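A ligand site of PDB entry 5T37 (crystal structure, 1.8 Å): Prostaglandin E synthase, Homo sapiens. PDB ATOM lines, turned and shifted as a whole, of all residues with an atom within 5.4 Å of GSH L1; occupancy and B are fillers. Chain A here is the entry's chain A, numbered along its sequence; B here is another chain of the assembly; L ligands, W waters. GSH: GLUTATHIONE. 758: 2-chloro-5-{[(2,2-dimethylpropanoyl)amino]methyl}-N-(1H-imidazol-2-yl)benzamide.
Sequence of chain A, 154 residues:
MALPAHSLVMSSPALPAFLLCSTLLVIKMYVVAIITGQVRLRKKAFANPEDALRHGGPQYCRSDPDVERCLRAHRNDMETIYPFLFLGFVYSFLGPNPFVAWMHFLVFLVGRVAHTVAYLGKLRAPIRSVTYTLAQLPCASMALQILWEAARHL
A nitrogen (N20) of 758 L2 sits close to a sulfur (SG2) of GSH L1 (3.6 Å).
The side-chain amide oxygen of Asn 76 lies close to a ring nitrogen (NE2) of His 115. The guanidinium group (NH1) of Arg 75 is in hydrogen-bond range of the backbone carbonyl oxygen (O) of Leu 71 of chain B (2.5 Å). The side-chain hydroxyl of Tyr 119 is in hydrogen-bond range of the side-chain amide nitrogen of Asn 48 of chain B, 3.1 Å away. The guanidinium group of Arg 72 lies within hydrogen-bond range of the side-chain hydroxyl of Tyr 119 (3.1 Å). The guanidinium group of Arg 72 lies within hydrogen-bond range of the side-chain amide oxygen of Asn 48 of chain B (2.8 Å). The guanidinium group (NH1) of Arg 128 lies close to the side-chain amide nitrogen (ND2) of Asn 48 of chain B (3.4 Å). The side-chain carboxylate (OE2) of Glu 79 is in salt-bridge range of the guanidinium group (NE) of Arg 75, at 2.8 Å.
OH of Tyr 119 lies within hydrogen-bond range of O32 of GSH L1, at 2.6 Å. A sulfur (SG2) of GSH L1 lies close to the side-chain hydroxyl (OG) of Ser 129 (3.2 Å). A ring nitrogen (NE2) of His 115 sits at hydrogen-bond distance from an oxygen (O2) of GSH L1. The side-chain amide nitrogen (ND2) of Asn 76 lies within hydrogen-bond range of an oxygen (O31) of GSH L1 (2.9 Å). A nitrogen (N19) of 758 L2 sits at hydrogen-bond distance from the side-chain hydroxyl (OG) of Ser 129 (2.8 Å). An oxygen (O2) of GSH L1 sits at hydrogen-bond distance from the guanidinium group of Arg 128 (2.8 Å). The side-chain carboxylate (OE1) of Glu 79 is in salt-bridge range of a nitrogen (N1) of GSH L1, 2.9 Å away. The guanidinium group of Arg 40 of chain B lies within salt-bridge range of an oxygen (O12) of GSH L1 (3.0 Å).
Water W2 bridges an oxygen (OE1) of GSH L1 (2.6 Å) and the side-chain carboxylate (OE1) of Glu 79 (2.7 Å). Water W4 lies within hydrogen-bond range of O32 of GSH L1 (2.7 Å) and NH2 of Arg 40 of chain B (3.3 Å). Water W3 lies within hydrogen-bond range of a nitrogen (N1) of GSH L1 (2.8 Å), a ring nitrogen (ND1) of His 74 of chain B (2.8 Å) and the side-chain hydroxyl (OG1) of Thr 36 of chain B (3.0 Å). Water W1 lies within hydrogen-bond range of O11 of GSH L1 and NE of Arg 40 of chain B.
CB of Arg 72 touches O32 of GSH L1, at 3.6 Å. Tyr 132 touches GSH L1 (CE2 to OE1, 3.2 Å). Ala 33 of chain B touches GSH L1 (O to CG1, 3.4 Å). CG2 of Thr 36 of chain B touches O12 of GSH L1 (3.5 Å). CD2 of Leu 71 of chain B touches O12 of GSH L1 (3.5 Å). Hydrophobic or aromatic side chains within 4 Å of GSH L1: His 115, Tyr 119, Tyr 132 and Leu 71 of chain B. Within 4 Å of GSH L1: Arg 72, Asn 76, Glu 79, His 115, Tyr 119, Arg 128, Ser 129, Tyr 132, Ala 33 of chain B, Thr 36 of chain B, Arg 40 of chain B and Leu 71 of chain B.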
ATOM      1  N   ARG A  72       2.694 -30.970 -35.485  1.00  0.00           N
ATOM      2  CA  ARG A  72       3.242 -29.940 -34.599  1.00  0.00           C
ATOM      3  C   ARG A  72       4.495 -29.280 -35.178  1.00  0.00           C
ATOM      4  O   ARG A  72       4.655 -28.059 -35.061  1.00  0.00           O
ATOM      5  CB  ARG A  72       3.551 -30.514 -33.205  1.00  0.00           C
ATOM      6  CG  ARG A  72       2.310 -30.776 -32.349  1.00  0.00           C
ATOM      7  CD  ARG A  72       2.643 -30.969 -30.871  1.00  0.00           C
ATOM      8  NE  ARG A  72       3.519 -32.127 -30.629  1.00  0.00           N
ATOM      9  CZ  ARG A  72       3.108 -33.386 -30.564  1.00  0.00           C
ATOM     10  NH1 ARG A  72       1.833 -33.693 -30.732  1.00  0.00           N
ATOM     11  NH2 ARG A  72       3.987 -34.355 -30.338  1.00  0.00           N
ATOM     12  N   ALA A  73       5.358 -30.079 -35.802  1.00  0.00           N
ATOM     13  CA  ALA A  73       6.553 -29.548 -36.451  1.00  0.00           C
ATOM     14  C   ALA A  73       6.171 -28.630 -37.605  1.00  0.00           C
ATOM     15  O   ALA A  73       6.725 -27.533 -37.755  1.00  0.00           O
ATOM     16  CB  ALA A  73       7.450 -30.682 -36.933  1.00  0.00           C
ATOM     17  N   ARG A  75       3.243 -27.073 -37.970  1.00  0.00           N
ATOM     18  CA  ARG A  75       2.607 -25.875 -37.416  1.00  0.00           C
ATOM     19  C   ARG A  75       3.645 -24.887 -36.872  1.00  0.00           C
ATOM     20  O   ARG A  75       3.543 -23.682 -37.122  1.00  0.00           O
ATOM     21  CB  ARG A  75       1.574 -26.214 -36.337  1.00  0.00           C
ATOM     22  CG  ARG A  75       0.975 -24.965 -35.717  1.00  0.00           C
ATOM     23  CD  ARG A  75      -0.178 -25.246 -34.789  1.00  0.00           C
ATOM     24  NE  ARG A  75      -0.560 -24.013 -34.103  1.00  0.00           N
ATOM     25  CZ  ARG A  75      -1.721 -23.809 -33.478  1.00  0.00           C
ATOM     26  NH1 ARG A  75      -1.954 -22.648 -32.904  1.00  0.00           N
ATOM     27  NH2 ARG A  75      -2.641 -24.770 -33.427  1.00  0.00           N
ATOM     28  N   ASN A  76       4.642 -25.389 -36.150  1.00  0.00           N
ATOM     29  CA  ASN A  76       5.695 -24.520 -35.630  1.00  0.00           C
ATOM     30  C   ASN A  76       6.452 -23.818 -36.755  1.00  0.00           C
ATOM     31  O   ASN A  76       6.798 -22.634 -36.634  1.00  0.00           O
ATOM     32  CB  ASN A  76       6.648 -25.262 -34.694  1.00  0.00           C
ATOM     33  CG  ASN A  76       7.549 -24.328 -33.906  1.00  0.00           C
ATOM     34  OD1 ASN A  76       8.596 -23.904 -34.396  1.00  0.00           O
ATOM     35  ND2 ASN A  76       7.129 -23.990 -32.697  1.00  0.00           N
ATOM     36  N   GLU A  79       4.404 -20.984 -37.787  1.00  0.00           N
ATOM     37  CA  GLU A  79       4.483 -19.937 -36.760  1.00  0.00           C
ATOM     38  C   GLU A  79       5.786 -19.131 -36.804  1.00  0.00           C
ATOM     39  O   GLU A  79       5.880 -18.078 -36.174  1.00  0.00           O
ATOM     40  CB  GLU A  79       4.269 -20.542 -35.363  1.00  0.00           C
ATOM     41  CG  GLU A  79       2.867 -21.095 -35.134  1.00  0.00           C
ATOM     42  CD  GLU A  79       2.699 -21.852 -33.812  1.00  0.00           C
ATOM     43  OE1 GLU A  79       3.693 -22.029 -33.073  1.00  0.00           O
ATOM     44  OE2 GLU A  79       1.561 -22.275 -33.518  1.00  0.00           O
ATOM     45  N   HIS A 115      15.739 -27.476 -35.724  1.00  0.00           N
ATOM     46  CA  HIS A 115      14.447 -27.601 -35.032  1.00  0.00           C
ATOM     47  C   HIS A 115      13.645 -28.799 -35.535  1.00  0.00           C
ATOM     48  O   HIS A 115      13.129 -29.575 -34.726  1.00  0.00           O
ATOM     49  CB  HIS A 115      13.629 -26.311 -35.184  1.00  0.00           C
ATOM     50  CG  HIS A 115      12.359 -26.303 -34.391  1.00  0.00           C
ATOM     51  ND1 HIS A 115      11.176 -26.847 -34.865  1.00  0.00           N
ATOM     52  CD2 HIS A 115      12.074 -25.823 -33.160  1.00  0.00           C
ATOM     53  CE1 HIS A 115      10.229 -26.700 -33.957  1.00  0.00           C
ATOM     54  NE2 HIS A 115      10.755 -26.083 -32.907  1.00  0.00           N
ATOM     55  N   TYR A 119      12.772 -32.115 -33.530  1.00  0.00           N
ATOM     56  CA  TYR A 119      11.360 -32.419 -33.292  1.00  0.00           C
ATOM     57  C   TYR A 119      10.985 -33.815 -33.772  1.00  0.00           C
ATOM     58  O   TYR A 119      10.474 -34.627 -33.003  1.00  0.00           O
ATOM     59  CB  TYR A 119      10.440 -31.387 -33.974  1.00  0.00           C
ATOM     60  CG  TYR A 119       9.208 -31.044 -33.157  1.00  0.00           C
ATOM     61  CD1 TYR A 119       8.752 -31.894 -32.142  1.00  0.00           C
ATOM     62  CD2 TYR A 119       8.487 -29.875 -33.396  1.00  0.00           C
ATOM     63  CE1 TYR A 119       7.639 -31.591 -31.388  1.00  0.00           C
ATOM     64  CE2 TYR A 119       7.361 -29.555 -32.648  1.00  0.00           C
ATOM     65  CZ  TYR A 119       6.944 -30.418 -31.637  1.00  0.00           C
ATOM     66  OH  TYR A 119       5.844 -30.131 -30.875  1.00  0.00           O
ATOM     67  N   ARG A 128      15.246 -29.014 -28.853  1.00  0.00           N
ATOM     68  CA  ARG A 128      14.288 -28.380 -29.764  1.00  0.00           C
ATOM     69  C   ARG A 128      13.962 -26.950 -29.331  1.00  0.00           C
ATOM     70  O   ARG A 128      13.977 -26.026 -30.154  1.00  0.00           O
ATOM     71  CB  ARG A 128      12.996 -29.202 -29.863  1.00  0.00           C
ATOM     72  CG  ARG A 128      12.018 -28.681 -30.917  1.00  0.00           C
ATOM     73  CD  ARG A 128      10.588 -29.092 -30.613  1.00  0.00           C
ATOM     74  NE  ARG A 128      10.029 -28.392 -29.456  1.00  0.00           N
ATOM     75  CZ  ARG A 128       9.796 -28.952 -28.272  1.00  0.00           C
ATOM     76  NH1 ARG A 128      10.037 -30.242 -28.072  1.00  0.00           N
ATOM     77  NH2 ARG A 128       9.288 -28.219 -27.292  1.00  0.00           N
ATOM     78  N   SER A 129      13.686 -26.777 -28.044  1.00  0.00           N
ATOM     79  CA  SER A 129      13.357 -25.462 -27.494  1.00  0.00           C
ATOM     80  C   SER A 129      14.454 -24.433 -27.761  1.00  0.00           C
ATOM     81  O   SER A 129      14.160 -23.297 -28.140  1.00  0.00           O
ATOM     82  CB  SER A 129      13.052 -25.562 -25.987  1.00  0.00           C
ATOM     83  OG  SER A 129      12.495 -24.355 -25.502  1.00  0.00           O
ATOM     84  N   TYR A 132      14.572 -23.316 -31.456  1.00  0.00           N
ATOM     85  CA  TYR A 132      13.499 -22.346 -31.682  1.00  0.00           C
ATOM     86  C   TYR A 132      13.952 -20.941 -31.270  1.00  0.00           C
ATOM     87  O   TYR A 132      13.818 -19.992 -32.050  1.00  0.00           O
ATOM     88  CB  TYR A 132      12.220 -22.726 -30.921  1.00  0.00           C
ATOM     89  CG  TYR A 132      11.194 -21.620 -30.843  1.00  0.00           C
ATOM     90  CD1 TYR A 132      11.102 -20.787 -29.727  1.00  0.00           C
ATOM     91  CD2 TYR A 132      10.318 -21.389 -31.906  1.00  0.00           C
ATOM     92  CE1 TYR A 132      10.171 -19.757 -29.652  1.00  0.00           C
ATOM     93  CE2 TYR A 132       9.373 -20.365 -31.848  1.00  0.00           C
ATOM     94  CZ  TYR A 132       9.303 -19.554 -30.725  1.00  0.00           C
ATOM     95  OH  TYR A 132       8.373 -18.545 -30.674  1.00  0.00           O
ATOM     96  N   ALA B  33       3.227 -16.428 -28.962  1.00  0.00           N
ATOM     97  CA  ALA B  33       4.069 -17.621 -28.884  1.00  0.00           C
ATOM     98  C   ALA B  33       4.774 -17.739 -27.528  1.00  0.00           C
ATOM     99  O   ALA B  33       4.803 -18.813 -26.930  1.00  0.00           O
ATOM    100  CB  ALA B  33       5.092 -17.634 -30.020  1.00  0.00           C
ATOM    101  N   ILE B  34       5.327 -16.620 -27.054  1.00  0.00           N
ATOM    102  CA  ILE B  34       6.000 -16.573 -25.751  1.00  0.00           C
ATOM    103  C   ILE B  34       5.022 -16.847 -24.609  1.00  0.00           C
ATOM    104  O   ILE B  34       5.314 -17.648 -23.718  1.00  0.00           O
ATOM    105  CB  ILE B  34       6.762 -15.232 -25.546  1.00  0.00           C
ATOM    106  CG1 ILE B  34       7.955 -15.148 -26.503  1.00  0.00           C
ATOM    107  CG2 ILE B  34       7.235 -15.075 -24.089  1.00  0.00           C
ATOM    108  CD1 ILE B  34       8.539 -13.754 -26.678  1.00  0.00           C
ATOM    109  N   THR B  36       2.235 -18.525 -24.805  1.00  0.00           N
ATOM    110  CA  THR B  36       1.893 -19.947 -24.927  1.00  0.00           C
ATOM    111  C   THR B  36       2.919 -20.826 -24.197  1.00  0.00           C
ATOM    112  O   THR B  36       2.542 -21.684 -23.402  1.00  0.00           O
ATOM    113  CB  THR B  36       1.776 -20.393 -26.415  1.00  0.00           C
ATOM    114  OG1 THR B  36       0.863 -19.534 -27.106  1.00  0.00           O
ATOM    115  CG2 THR B  36       1.271 -21.837 -26.507  1.00  0.00           C
ATOM    116  N   GLY B  37       4.205 -20.586 -24.463  1.00  0.00           N
ATOM    117  CA  GLY B  37       5.293 -21.322 -23.811  1.00  0.00           C
ATOM    118  C   GLY B  37       5.296 -21.178 -22.295  1.00  0.00           C
ATOM    119  O   GLY B  37       5.489 -22.151 -21.568  1.00  0.00           O
ATOM    120  N   ARG B  40       2.434 -23.162 -20.793  1.00  0.00           N
ATOM    121  CA  ARG B  40       2.820 -24.582 -20.789  1.00  0.00           C
ATOM    122  C   ARG B  40       3.673 -24.920 -19.581  1.00  0.00           C
ATOM    123  O   ARG B  40       3.454 -25.940 -18.927  1.00  0.00           O
ATOM    124  CB  ARG B  40       3.571 -24.952 -22.070  1.00  0.00           C
ATOM    125  CG  ARG B  40       2.716 -25.052 -23.328  1.00  0.00           C
ATOM    126  CD  ARG B  40       3.493 -25.730 -24.458  1.00  0.00           C
ATOM    127  NE  ARG B  40       2.715 -25.894 -25.686  1.00  0.00           N
ATOM    128  CZ  ARG B  40       1.844 -26.879 -25.910  1.00  0.00           C
ATOM    129  NH1 ARG B  40       1.609 -27.796 -24.984  1.00  0.00           N
ATOM    130  NH2 ARG B  40       1.204 -26.934 -27.068  1.00  0.00           N
ATOM    131  N   ALA B  47       3.194 -30.721 -24.942  1.00  0.00           N
ATOM    132  CA  ALA B  47       2.695 -31.484 -26.090  1.00  0.00           C
ATOM    133  C   ALA B  47       3.546 -32.718 -26.351  1.00  0.00           C
ATOM    134  O   ALA B  47       3.101 -33.663 -27.002  1.00  0.00           O
ATOM    135  CB  ALA B  47       2.633 -30.598 -27.325  1.00  0.00           C
ATOM    136  N   ASN B  48       4.768 -32.716 -25.833  1.00  0.00           N
ATOM    137  CA  ASN B  48       5.755 -33.750 -26.123  1.00  0.00           C
ATOM    138  C   ASN B  48       6.241 -34.473 -24.873  1.00  0.00           C
ATOM    139  O   ASN B  48       6.517 -33.834 -23.857  1.00  0.00           O
ATOM    140  CB  ASN B  48       6.947 -33.154 -26.865  1.00  0.00           C
ATOM    141  CG  ASN B  48       6.521 -32.362 -28.094  1.00  0.00           C
ATOM    142  OD1 ASN B  48       6.017 -32.932 -29.059  1.00  0.00           O
ATOM    143  ND2 ASN B  48       6.723 -31.054 -28.049  1.00  0.00           N
ATOM    144  N   VAL B  67      -3.691 -23.436 -22.496  1.00  0.00           N
ATOM    145  CA  VAL B  67      -2.754 -23.701 -23.595  1.00  0.00           C
ATOM    146  C   VAL B  67      -3.499 -23.777 -24.931  1.00  0.00           C
ATOM    147  O   VAL B  67      -3.079 -23.149 -25.909  1.00  0.00           O
ATOM    148  CB  VAL B  67      -1.918 -24.990 -23.363  1.00  0.00           C
ATOM    149  CG1 VAL B  67      -1.023 -25.280 -24.570  1.00  0.00           C
ATOM    150  CG2 VAL B  67      -1.062 -24.867 -22.095  1.00  0.00           C
ATOM    151  N   LEU B  71      -3.168 -21.404 -28.285  1.00  0.00           N
ATOM    152  CA  LEU B  71      -2.972 -21.991 -29.615  1.00  0.00           C
ATOM    153  C   LEU B  71      -4.026 -21.519 -30.611  1.00  0.00           C
ATOM    154  O   LEU B  71      -3.718 -21.273 -31.767  1.00  0.00           O
ATOM    155  CB  LEU B  71      -2.924 -23.519 -29.553  1.00  0.00           C
ATOM    156  CG  LEU B  71      -1.686 -24.150 -28.910  1.00  0.00           C
ATOM    157  CD1 LEU B  71      -1.917 -25.622 -28.645  1.00  0.00           C
ATOM    158  CD2 LEU B  71      -0.446 -23.956 -29.794  1.00  0.00           C
ATOM    159  N   HIS B  74      -3.226 -17.915 -31.573  1.00  0.00           N
ATOM    160  CA  HIS B  74      -2.094 -17.957 -32.499  1.00  0.00           C
ATOM    161  C   HIS B  74      -2.534 -18.437 -33.884  1.00  0.00           C
ATOM    162  O   HIS B  74      -2.125 -17.854 -34.902  1.00  0.00           O
ATOM    163  CB  HIS B  74      -0.973 -18.850 -31.952  1.00  0.00           C
ATOM    164  CG  HIS B  74       0.389 -18.525 -32.502  1.00  0.00           C
ATOM    165  ND1 HIS B  74       1.547 -18.957 -31.905  1.00  0.00           N
ATOM    166  CD2 HIS B  74       0.766 -17.800 -33.582  1.00  0.00           C
ATOM    167  CE1 HIS B  74       2.584 -18.528 -32.596  1.00  0.00           C
ATOM    168  NE2 HIS B  74       2.145 -17.821 -33.613  1.00  0.00           N
HETATM  169  N1  GSH L   1       2.848 -22.897 -30.466  1.00  0.00           N
HETATM  170  CA1 GSH L   1       4.058 -23.072 -29.674  1.00  0.00           C
HETATM  171  C1  GSH L   1       3.832 -24.122 -28.609  1.00  0.00           C
HETATM  172  O11 GSH L   1       4.819 -24.658 -28.049  1.00  0.00           O
HETATM  173  O12 GSH L   1       2.689 -24.490 -28.289  1.00  0.00           O
HETATM  174  CB1 GSH L   1       4.447 -21.721 -29.067  1.00  0.00           C
HETATM  175  CG1 GSH L   1       5.785 -21.713 -28.328  1.00  0.00           C
HETATM  176  CD1 GSH L   1       6.894 -22.301 -29.175  1.00  0.00           C
HETATM  177  OE1 GSH L   1       6.986 -21.992 -30.543  1.00  0.00           O
HETATM  178  N2  GSH L   1       7.745 -23.114 -28.558  1.00  0.00           N
HETATM  179  CA2 GSH L   1       8.813 -23.800 -29.262  1.00  0.00           C
HETATM  180  C2  GSH L   1       8.397 -25.136 -29.820  1.00  0.00           C
HETATM  181  O2  GSH L   1       9.333 -25.895 -30.533  1.00  0.00           O
HETATM  182  CB2 GSH L   1      10.012 -23.982 -28.336  1.00  0.00           C
HETATM  183  SG2 GSH L   1       9.592 -24.860 -26.811  1.00  0.00           S
HETATM  184  N3  GSH L   1       7.142 -25.530 -29.609  1.00  0.00           N
HETATM  185  CA3 GSH L   1       6.667 -26.835 -30.056  1.00  0.00           C
HETATM  186  C3  GSH L   1       5.453 -26.739 -30.957  1.00  0.00           C
HETATM  187  O31 GSH L   1       5.097 -25.642 -31.439  1.00  0.00           O
HETATM  188  O32 GSH L   1       4.802 -27.769 -31.247  1.00  0.00           O
HETATM  189  C7  758 L   2       8.907 -24.660 -23.194  1.00  0.00           C
HETATM  190  C6  758 L   2      11.007 -25.706 -22.608  1.00  0.00           C
HETATM  191  C1  758 L   2       8.377 -25.906 -23.513  1.00  0.00           C
HETATM  192  C5  758 L   2      16.439 -24.193 -21.526  1.00  0.00           C
HETATM  193  C4  758 L   2      16.414 -23.279 -22.555  1.00  0.00           C
HETATM  194  C3  758 L   2      10.234 -24.559 -22.740  1.00  0.00           C
HETATM  195  C2  758 L   2       9.146 -27.061 -23.375  1.00  0.00           C
HETATM  196  C8  758 L   2      10.464 -26.955 -22.922  1.00  0.00           C
HETATM  197  C9  758 L   2      14.475 -24.178 -22.542  1.00  0.00           C
HETATM  198  C10 758 L   2      12.371 -25.535 -22.114  1.00  0.00           C
HETATM  199  C11 758 L   2       8.854 -21.147 -23.968  1.00  0.00           C
HETATM  200  C12 758 L   2      10.775 -20.921 -25.608  1.00  0.00           C
HETATM  201  C13 758 L   2       8.476 -20.154 -26.252  1.00  0.00           C
HETATM  202  C14 758 L   2       9.761 -18.870 -24.549  1.00  0.00           C
HETATM  203  C15 758 L   2       8.087 -23.416 -23.350  1.00  0.00           C
HETATM  204  C16 758 L   2       9.474 -20.280 -25.085  1.00  0.00           C
HETATM  205  N17 758 L   2      15.186 -23.284 -23.181  1.00  0.00           N
HETATM  206  N18 758 L   2      15.191 -24.761 -21.524  1.00  0.00           N
HETATM  207  N19 758 L   2      13.133 -24.573 -22.791  1.00  0.00           N
HETATM  208  N20 758 L   2       8.653 -22.483 -24.295  1.00  0.00           N
HETATM  209  O21 758 L   2      12.800 -26.186 -21.157  1.00  0.00           O
HETATM  210  O22 758 L   2       8.555 -20.686 -22.870  1.00  0.00           O
HETATM  211 CL23 758 L   2      11.381 -28.415 -22.761  1.00  0.00          CL
HETATM  212  O   HOH W   1       4.481 -27.558 -27.666  1.00  0.00           O
HETATM  213  O   HOH W   2       5.738 -20.425 -32.260  1.00  0.00           O
HETATM  214  O   HOH W   3       1.208 -20.756 -29.805  1.00  0.00           O
HETATM  215  O   HOH W   4       2.393 -27.662 -30.051  1.00  0.00           O
